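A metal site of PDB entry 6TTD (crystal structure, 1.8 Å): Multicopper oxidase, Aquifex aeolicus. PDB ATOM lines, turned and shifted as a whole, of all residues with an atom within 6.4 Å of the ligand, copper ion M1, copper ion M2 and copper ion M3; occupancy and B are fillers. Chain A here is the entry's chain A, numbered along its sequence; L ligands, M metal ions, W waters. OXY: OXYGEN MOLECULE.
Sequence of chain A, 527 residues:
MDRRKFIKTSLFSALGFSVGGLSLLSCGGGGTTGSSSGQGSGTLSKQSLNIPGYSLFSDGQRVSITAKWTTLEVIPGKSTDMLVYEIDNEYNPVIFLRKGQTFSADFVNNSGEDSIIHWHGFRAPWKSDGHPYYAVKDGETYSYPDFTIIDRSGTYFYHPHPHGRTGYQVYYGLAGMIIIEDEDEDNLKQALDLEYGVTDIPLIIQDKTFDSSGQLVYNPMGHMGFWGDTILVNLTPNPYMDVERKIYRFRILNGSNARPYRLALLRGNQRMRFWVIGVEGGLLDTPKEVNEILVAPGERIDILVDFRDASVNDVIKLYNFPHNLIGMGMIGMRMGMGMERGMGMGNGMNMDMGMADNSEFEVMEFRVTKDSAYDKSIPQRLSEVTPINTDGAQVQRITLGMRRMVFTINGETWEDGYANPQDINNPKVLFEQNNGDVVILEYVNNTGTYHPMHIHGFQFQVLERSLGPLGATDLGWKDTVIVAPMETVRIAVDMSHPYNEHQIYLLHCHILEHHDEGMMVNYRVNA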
ATOM      1  N   HIS A 118      19.359   6.494 -28.546  1.00  0.00           N
ATOM      2  CA  HIS A 118      19.684   7.087 -27.255  1.00  0.00           C
ATOM      3  C   HIS A 118      20.720   8.203 -27.453  1.00  0.00           C
ATOM      4  O   HIS A 118      21.655   8.068 -28.271  1.00  0.00           O
ATOM      5  CB  HIS A 118      20.235   5.983 -26.325  1.00  0.00           C
ATOM      6  CG  HIS A 118      20.981   6.476 -25.108  1.00  0.00           C
ATOM      7  ND1 HIS A 118      20.388   7.223 -24.124  1.00  0.00           N
ATOM      8  CD2 HIS A 118      22.262   6.295 -24.723  1.00  0.00           C
ATOM      9  CE1 HIS A 118      21.272   7.489 -23.184  1.00  0.00           C
ATOM     10  NE2 HIS A 118      22.422   6.944 -23.526  1.00  0.00           N
ATOM     11  N   TRP A 119      20.533   9.326 -26.751  1.00  0.00           N
ATOM     12  CA  TRP A 119      21.443  10.469 -26.836  1.00  0.00           C
ATOM     13  C   TRP A 119      22.384  10.296 -25.651  1.00  0.00           C
ATOM     14  O   TRP A 119      22.114  10.725 -24.537  1.00  0.00           O
ATOM     15  CB  TRP A 119      20.692  11.802 -26.796  1.00  0.00           C
ATOM     16  CG  TRP A 119      19.360  11.675 -27.461  1.00  0.00           C
ATOM     17  CD1 TRP A 119      18.130  11.579 -26.837  1.00  0.00           C
ATOM     18  CD2 TRP A 119      19.085  11.581 -28.887  1.00  0.00           C
ATOM     19  NE1 TRP A 119      17.115  11.435 -27.812  1.00  0.00           N
ATOM     20  CE2 TRP A 119      17.687  11.436 -29.053  1.00  0.00           C
ATOM     21  CE3 TRP A 119      19.897  11.624 -30.039  1.00  0.00           C
ATOM     22  CZ2 TRP A 119      17.098  11.338 -30.307  1.00  0.00           C
ATOM     23  CZ3 TRP A 119      19.276  11.535 -31.309  1.00  0.00           C
ATOM     24  CH2 TRP A 119      17.916  11.391 -31.415  1.00  0.00           C
ATOM     25  N   HIS A 120      23.484   9.613 -25.884  1.00  0.00           N
ATOM     26  CA  HIS A 120      24.345   9.226 -24.765  1.00  0.00           C
ATOM     27  C   HIS A 120      25.038  10.481 -24.193  1.00  0.00           C
ATOM     28  O   HIS A 120      25.764  11.185 -24.897  1.00  0.00           O
ATOM     29  CB  HIS A 120      25.331   8.130 -25.230  1.00  0.00           C
ATOM     30  CG  HIS A 120      26.368   7.759 -24.208  1.00  0.00           C
ATOM     31  ND1 HIS A 120      26.892   6.475 -24.141  1.00  0.00           N
ATOM     32  CD2 HIS A 120      27.027   8.473 -23.261  1.00  0.00           C
ATOM     33  CE1 HIS A 120      27.815   6.419 -23.188  1.00  0.00           C
ATOM     34  NE2 HIS A 120      27.906   7.605 -22.633  1.00  0.00           N
ATOM     35  N   GLY A 121      24.788  10.764 -22.893  1.00  0.00           N
ATOM     36  CA  GLY A 121      25.316  11.931 -22.202  1.00  0.00           C
ATOM     37  C   GLY A 121      24.270  12.992 -21.924  1.00  0.00           C
ATOM     38  O   GLY A 121      24.509  13.840 -21.078  1.00  0.00           O
ATOM     39  N   ASP A 129      14.845   9.833 -23.734  1.00  0.00           N
ATOM     40  CA  ASP A 129      16.214   9.356 -23.557  1.00  0.00           C
ATOM     41  C   ASP A 129      16.545   8.177 -24.467  1.00  0.00           C
ATOM     42  O   ASP A 129      17.720   7.920 -24.734  1.00  0.00           O
ATOM     43  CB  ASP A 129      16.383   8.998 -22.067  1.00  0.00           C
ATOM     44  CG  ASP A 129      17.702   8.401 -21.722  1.00  0.00           C
ATOM     45  OD1 ASP A 129      18.750   8.969 -22.098  1.00  0.00           O
ATOM     46  OD2 ASP A 129      17.736   7.364 -20.994  1.00  0.00           O
ATOM     47  N   PHE A 157      27.127  11.541 -28.001  1.00  0.00           N
ATOM     48  CA  PHE A 157      27.170  10.285 -28.766  1.00  0.00           C
ATOM     49  C   PHE A 157      25.746   9.796 -29.007  1.00  0.00           C
ATOM     50  O   PHE A 157      25.005   9.599 -28.022  1.00  0.00           O
ATOM     51  CB  PHE A 157      27.998   9.282 -27.915  1.00  0.00           C
ATOM     52  CG  PHE A 157      28.220   7.870 -28.495  1.00  0.00           C
ATOM     53  CD1 PHE A 157      28.050   7.554 -29.842  1.00  0.00           C
ATOM     54  CD2 PHE A 157      28.696   6.869 -27.610  1.00  0.00           C
ATOM     55  CE1 PHE A 157      28.293   6.242 -30.310  1.00  0.00           C
ATOM     56  CE2 PHE A 157      28.936   5.575 -28.055  1.00  0.00           C
ATOM     57  CZ  PHE A 157      28.737   5.259 -29.419  1.00  0.00           C
ATOM     58  N   HIS A 159      23.325   6.712 -30.545  1.00  0.00           N
ATOM     59  CA  HIS A 159      23.430   5.341 -31.010  1.00  0.00           C
ATOM     60  C   HIS A 159      22.179   4.574 -30.572  1.00  0.00           C
ATOM     61  O   HIS A 159      21.453   5.045 -29.701  1.00  0.00           O
ATOM     62  CB  HIS A 159      24.712   4.682 -30.468  1.00  0.00           C
ATOM     63  CG  HIS A 159      24.720   4.453 -28.992  1.00  0.00           C
ATOM     64  ND1 HIS A 159      23.936   3.492 -28.385  1.00  0.00           N
ATOM     65  CD2 HIS A 159      25.463   5.004 -27.991  1.00  0.00           C
ATOM     66  CE1 HIS A 159      24.164   3.476 -27.075  1.00  0.00           C
ATOM     67  NE2 HIS A 159      25.098   4.376 -26.812  1.00  0.00           N
ATOM     68  N   PRO A 160      21.904   3.400 -31.171  1.00  0.00           N
ATOM     69  CA  PRO A 160      20.677   2.660 -30.821  1.00  0.00           C
ATOM     70  C   PRO A 160      20.760   2.001 -29.435  1.00  0.00           C
ATOM     71  O   PRO A 160      21.848   1.803 -28.875  1.00  0.00           O
ATOM     72  CB  PRO A 160      20.583   1.575 -31.908  1.00  0.00           C
ATOM     73  CG  PRO A 160      22.037   1.359 -32.318  1.00  0.00           C
ATOM     74  CD  PRO A 160      22.688   2.738 -32.229  1.00  0.00           C
ATOM     75  N   HIS A 161      19.591   1.623 -28.914  1.00  0.00           N
ATOM     76  CA  HIS A 161      19.570   1.043 -27.571  1.00  0.00           C
ATOM     77  C   HIS A 161      18.520  -0.075 -27.439  1.00  0.00           C
ATOM     78  O   HIS A 161      17.909  -0.191 -26.355  1.00  0.00           O
ATOM     79  CB  HIS A 161      19.278   2.187 -26.554  1.00  0.00           C
ATOM     80  CG  HIS A 161      20.060   2.072 -25.278  1.00  0.00           C
ATOM     81  ND1 HIS A 161      19.861   1.054 -24.368  1.00  0.00           N
ATOM     82  CD2 HIS A 161      21.036   2.862 -24.751  1.00  0.00           C
ATOM     83  CE1 HIS A 161      20.704   1.211 -23.357  1.00  0.00           C
ATOM     84  NE2 HIS A 161      21.412   2.318 -23.549  1.00  0.00           N
ATOM     85  N   THR A 166      21.837  -4.087 -29.051  1.00  0.00           N
ATOM     86  CA  THR A 166      22.564  -2.832 -29.218  1.00  0.00           C
ATOM     87  C   THR A 166      23.940  -3.078 -29.816  1.00  0.00           C
ATOM     88  O   THR A 166      24.404  -2.281 -30.641  1.00  0.00           O
ATOM     89  CB  THR A 166      22.662  -2.100 -27.869  1.00  0.00           C
ATOM     90  OG1 THR A 166      21.360  -1.652 -27.529  1.00  0.00           O
ATOM     91  CG2 THR A 166      23.593  -0.863 -27.942  1.00  0.00           C
ATOM     92  N   GLY A 298      32.063   4.235 -24.918  1.00  0.00           N
ATOM     93  CA  GLY A 298      31.206   5.175 -24.244  1.00  0.00           C
ATOM     94  C   GLY A 298      31.915   6.422 -23.771  1.00  0.00           C
ATOM     95  O   GLY A 298      31.260   7.450 -23.612  1.00  0.00           O
ATOM     96  N   HIS A 454      28.265   2.986 -17.025  1.00  0.00           N
ATOM     97  CA  HIS A 454      27.626   4.186 -17.532  1.00  0.00           C
ATOM     98  C   HIS A 454      26.274   4.327 -16.836  1.00  0.00           C
ATOM     99  O   HIS A 454      25.590   3.314 -16.596  1.00  0.00           O
ATOM    100  CB  HIS A 454      27.501   4.042 -19.057  1.00  0.00           C
ATOM    101  CG  HIS A 454      26.628   5.066 -19.688  1.00  0.00           C
ATOM    102  ND1 HIS A 454      26.855   6.425 -19.546  1.00  0.00           N
ATOM    103  CD2 HIS A 454      25.530   4.940 -20.504  1.00  0.00           C
ATOM    104  CE1 HIS A 454      25.940   7.086 -20.234  1.00  0.00           C
ATOM    105  NE2 HIS A 454      25.117   6.200 -20.800  1.00  0.00           N
ATOM    106  N   ILE A 455      25.882   5.552 -16.490  1.00  0.00           N
ATOM    107  CA  ILE A 455      24.507   5.833 -16.067  1.00  0.00           C
ATOM    108  C   ILE A 455      23.894   6.805 -17.045  1.00  0.00           C
ATOM    109  O   ILE A 455      24.565   7.721 -17.532  1.00  0.00           O
ATOM    110  CB  ILE A 455      24.372   6.372 -14.623  1.00  0.00           C
ATOM    111  CG1 ILE A 455      25.124   7.725 -14.463  1.00  0.00           C
ATOM    112  CG2 ILE A 455      24.887   5.346 -13.609  1.00  0.00           C
ATOM    113  CD1 ILE A 455      24.956   8.404 -13.043  1.00  0.00           C
ATOM    114  N   HIS A 456      22.618   6.580 -17.359  1.00  0.00           N
ATOM    115  CA  HIS A 456      21.829   7.590 -18.064  1.00  0.00           C
ATOM    116  C   HIS A 456      21.421   8.686 -17.062  1.00  0.00           C
ATOM    117  O   HIS A 456      21.450   8.483 -15.825  1.00  0.00           O
ATOM    118  CB  HIS A 456      20.572   6.947 -18.670  1.00  0.00           C
ATOM    119  CG  HIS A 456      20.842   5.950 -19.759  1.00  0.00           C
ATOM    120  ND1 HIS A 456      19.945   5.730 -20.803  1.00  0.00           N
ATOM    121  CD2 HIS A 456      21.880   5.109 -19.957  1.00  0.00           C
ATOM    122  CE1 HIS A 456      20.438   4.774 -21.596  1.00  0.00           C
ATOM    123  NE2 HIS A 456      21.606   4.386 -21.100  1.00  0.00           N
ATOM    124  N   GLY A 457      20.995   9.827 -17.600  1.00  0.00           N
ATOM    125  CA  GLY A 457      20.295  10.850 -16.846  1.00  0.00           C
ATOM    126  C   GLY A 457      21.150  11.933 -16.264  1.00  0.00           C
ATOM    127  O   GLY A 457      20.721  13.087 -16.229  1.00  0.00           O
ATOM    128  N   ASP A 479      30.489  10.466 -17.636  1.00  0.00           N
ATOM    129  CA  ASP A 479      29.276   9.651 -17.686  1.00  0.00           C
ATOM    130  C   ASP A 479      29.549   8.158 -17.877  1.00  0.00           C
ATOM    131  O   ASP A 479      28.612   7.359 -17.730  1.00  0.00           O
ATOM    132  CB  ASP A 479      28.259  10.184 -18.725  1.00  0.00           C
ATOM    133  CG  ASP A 479      28.617   9.837 -20.179  1.00  0.00           C
ATOM    134  OD1 ASP A 479      29.182   8.747 -20.459  1.00  0.00           O
ATOM    135  OD2 ASP A 479      28.312  10.682 -21.051  1.00  0.00           O
ATOM    136  N   THR A 480      30.816   7.764 -18.115  1.00  0.00           N
ATOM    137  CA  THR A 480      31.258   6.368 -18.189  1.00  0.00           C
ATOM    138  C   THR A 480      32.602   6.224 -17.465  1.00  0.00           C
ATOM    139  O   THR A 480      33.538   6.977 -17.753  1.00  0.00           O
ATOM    140  CB  THR A 480      31.422   5.950 -19.646  1.00  0.00           C
ATOM    141  OG1 THR A 480      30.151   6.099 -20.298  1.00  0.00           O
ATOM    142  CG2 THR A 480      31.873   4.515 -19.730  1.00  0.00           C
ATOM    143  N   LEU A 506      18.700   4.172 -16.916  1.00  0.00           N
ATOM    144  CA  LEU A 506      19.487   2.938 -16.906  1.00  0.00           C
ATOM    145  C   LEU A 506      20.825   3.128 -16.184  1.00  0.00           C
ATOM    146  O   LEU A 506      21.407   4.212 -16.175  1.00  0.00           O
ATOM    147  CB  LEU A 506      19.785   2.489 -18.341  1.00  0.00           C
ATOM    148  CG  LEU A 506      18.518   2.201 -19.118  1.00  0.00           C
ATOM    149  CD1 LEU A 506      18.925   1.882 -20.501  1.00  0.00           C
ATOM    150  CD2 LEU A 506      17.900   0.960 -18.476  1.00  0.00           C
ATOM    151  N   HIS A 508      24.330   0.721 -16.553  1.00  0.00           N
ATOM    152  CA  HIS A 508      24.728  -0.512 -17.220  1.00  0.00           C
ATOM    153  C   HIS A 508      26.179  -0.442 -17.685  1.00  0.00           C
ATOM    154  O   HIS A 508      26.822   0.614 -17.688  1.00  0.00           O
ATOM    155  CB  HIS A 508      23.831  -0.808 -18.436  1.00  0.00           C
ATOM    156  CG  HIS A 508      23.962   0.185 -19.569  1.00  0.00           C
ATOM    157  ND1 HIS A 508      24.935   0.089 -20.564  1.00  0.00           N
ATOM    158  CD2 HIS A 508      23.186   1.251 -19.902  1.00  0.00           C
ATOM    159  CE1 HIS A 508      24.763   1.077 -21.431  1.00  0.00           C
ATOM    160  NE2 HIS A 508      23.703   1.790 -21.070  1.00  0.00           N
ATOM    161  N   CYS A 509      26.687  -1.605 -18.057  1.00  0.00           N
ATOM    162  CA  CYS A 509      28.014  -1.699 -18.643  1.00  0.00           C
ATOM    163  C   CYS A 509      27.962  -1.262 -20.100  1.00  0.00           C
ATOM    164  O   CYS A 509      26.989  -1.547 -20.829  1.00  0.00           O
ATOM    165  CB  CYS A 509      28.534  -3.141 -18.522  1.00  0.00           C
ATOM    166  SG  CYS A 509      30.145  -3.316 -19.199  1.00  0.00           S
ATOM    167  N   HIS A 510      29.012  -0.547 -20.539  1.00  0.00           N
ATOM    168  CA  HIS A 510      29.038  -0.114 -21.925  1.00  0.00           C
ATOM    169  C   HIS A 510      29.902  -1.003 -22.822  1.00  0.00           C
ATOM    170  O   HIS A 510      30.176  -0.635 -23.958  1.00  0.00           O
ATOM    171  CB  HIS A 510      29.484   1.332 -22.018  1.00  0.00           C
ATOM    172  CG  HIS A 510      28.884   2.051 -23.187  1.00  0.00           C
ATOM    173  ND1 HIS A 510      29.291   1.834 -24.480  1.00  0.00           N
ATOM    174  CD2 HIS A 510      27.896   2.987 -23.252  1.00  0.00           C
ATOM    175  CE1 HIS A 510      28.602   2.621 -25.292  1.00  0.00           C
ATOM    176  NE2 HIS A 510      27.756   3.334 -24.570  1.00  0.00           N
ATOM    177  N   LEU A 512      29.136  -3.473 -25.164  1.00  0.00           N
ATOM    178  CA  LEU A 512      27.790  -3.656 -25.729  1.00  0.00           C
ATOM    179  C   LEU A 512      27.306  -5.127 -25.678  1.00  0.00           C
ATOM    180  O   LEU A 512      26.100  -5.368 -25.480  1.00  0.00           O
ATOM    181  CB  LEU A 512      27.743  -3.109 -27.153  1.00  0.00           C
ATOM    182  CG  LEU A 512      28.060  -1.617 -27.288  1.00  0.00           C
ATOM    183  CD1 LEU A 512      27.815  -1.150 -28.773  1.00  0.00           C
ATOM    184  CD2 LEU A 512      27.307  -0.740 -26.319  1.00  0.00           C
ATOM    185  N   HIS A 515      26.046  -5.395 -22.112  1.00  0.00           N
ATOM    186  CA  HIS A 515      24.716  -4.780 -22.149  1.00  0.00           C
ATOM    187  C   HIS A 515      23.700  -5.745 -22.754  1.00  0.00           C
ATOM    188  O   HIS A 515      22.666  -6.030 -22.140  1.00  0.00           O
ATOM    189  CB  HIS A 515      24.741  -3.453 -22.941  1.00  0.00           C
ATOM    190  CG  HIS A 515      23.383  -2.957 -23.321  1.00  0.00           C
ATOM    191  ND1 HIS A 515      22.678  -3.464 -24.400  1.00  0.00           N
ATOM    192  CD2 HIS A 515      22.578  -2.031 -22.758  1.00  0.00           C
ATOM    193  CE1 HIS A 515      21.502  -2.868 -24.483  1.00  0.00           C
ATOM    194  NE2 HIS A 515      21.417  -1.993 -23.491  1.00  0.00           N
ATOM    195  N   MET A 520      22.644  -4.735 -16.908  1.00  0.00           N
ATOM    196  CA  MET A 520      21.904  -3.474 -17.011  1.00  0.00           C
ATOM    197  C   MET A 520      20.752  -3.541 -16.019  1.00  0.00           C
ATOM    198  O   MET A 520      20.168  -4.606 -15.841  1.00  0.00           O
ATOM    199  CB  MET A 520      21.356  -3.304 -18.425  1.00  0.00           C
ATOM    200  CG  MET A 520      20.408  -2.171 -18.595  1.00  0.00           C
ATOM    201  SD  MET A 520      19.949  -1.862 -20.365  1.00  0.00           S
ATOM    202  CE  MET A 520      19.333  -3.470 -20.868  1.00  0.00           C
HETATM  203  O1  OXY L   1      24.440   3.469 -23.704  1.00  0.00           O
HETATM  204  O2  OXY L   1      24.505   4.549 -23.498  1.00  0.00           O
HETATM  205 CU    CU M   1      26.278   4.830 -25.197  1.00  0.00          CU
HETATM  206 CU    CU M   2      22.673   3.143 -22.251  1.00  0.00          CU
HETATM  207 CU    CU M   3      23.818   6.465 -22.199  1.00  0.00          CU
HETATM  208  O   HOH W   1      23.296   9.235 -20.916  1.00  0.00           O
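A ring nitrogen (NE2) of His 454 binds copper ion M3 (1.9 Å).
Copper ion M3 is bound by NE2 of His 118, at 2.0 Å.
O2 of the ligand is bound to copper ion M3 (2.4 Å).
Within 4 Å of copper ion M3: His 118, His 120, His 454 and His 456.
Copper ion M1 is bound by ND1 of His 120, NE2 of His 159, NE2 of His 510 and O2 of the ligand.
Within 4 Å of the ligand: His 118, His 120, His 159, His 161, His 454, His 456, His 508 and His 510.
CE2 of Phe 157 touches copper ion M1, at 3.97 Å.
Within 4 Å of copper ion M1: His 120, Phe 157, His 159 and His 510.
Copper ion M2 is bound by NE2 of His 161, NE2 of His 456, NE2 of His 508 and O1 of the ligand.
NE2 of His 120 lies within hydrogen-bond range of OD1 of Asp 479 (2.8 Å).
The backbone carbonyl oxygen (O) of Leu 506 lies within hydrogen-bond range of the backbone NH (N) of His 456 (2.9 Å).
The backbone carbonyl oxygen (O) of His 508 sits at hydrogen-bond distance from the backbone NH (N) of His 454, 2.9 Å away.
The backbone NH (N) of His 118 sits at hydrogen-bond distance from the backbone carbonyl oxygen (O) of His 159 (2.8 Å).
The side-chain hydroxyl (OG1) of Thr 480 lies within hydrogen-bond range of a ring nitrogen (ND1) of His 454.
ND1 of His 454 is in hydrogen-bond range of O of Asp 479 (2.7 Å).
The side-chain carboxylate of Asp 129 lies within hydrogen-bond range of a ring nitrogen (ND1) of His 456 (2.8 Å).
A ring nitrogen (ND1) of His 118 is in hydrogen-bond range of the backbone carbonyl oxygen (O) of Asp 129 (2.8 Å).
Four residues have an atom within 4 Å of copper ion M2: His 161, His 454, His 456 and His 508.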
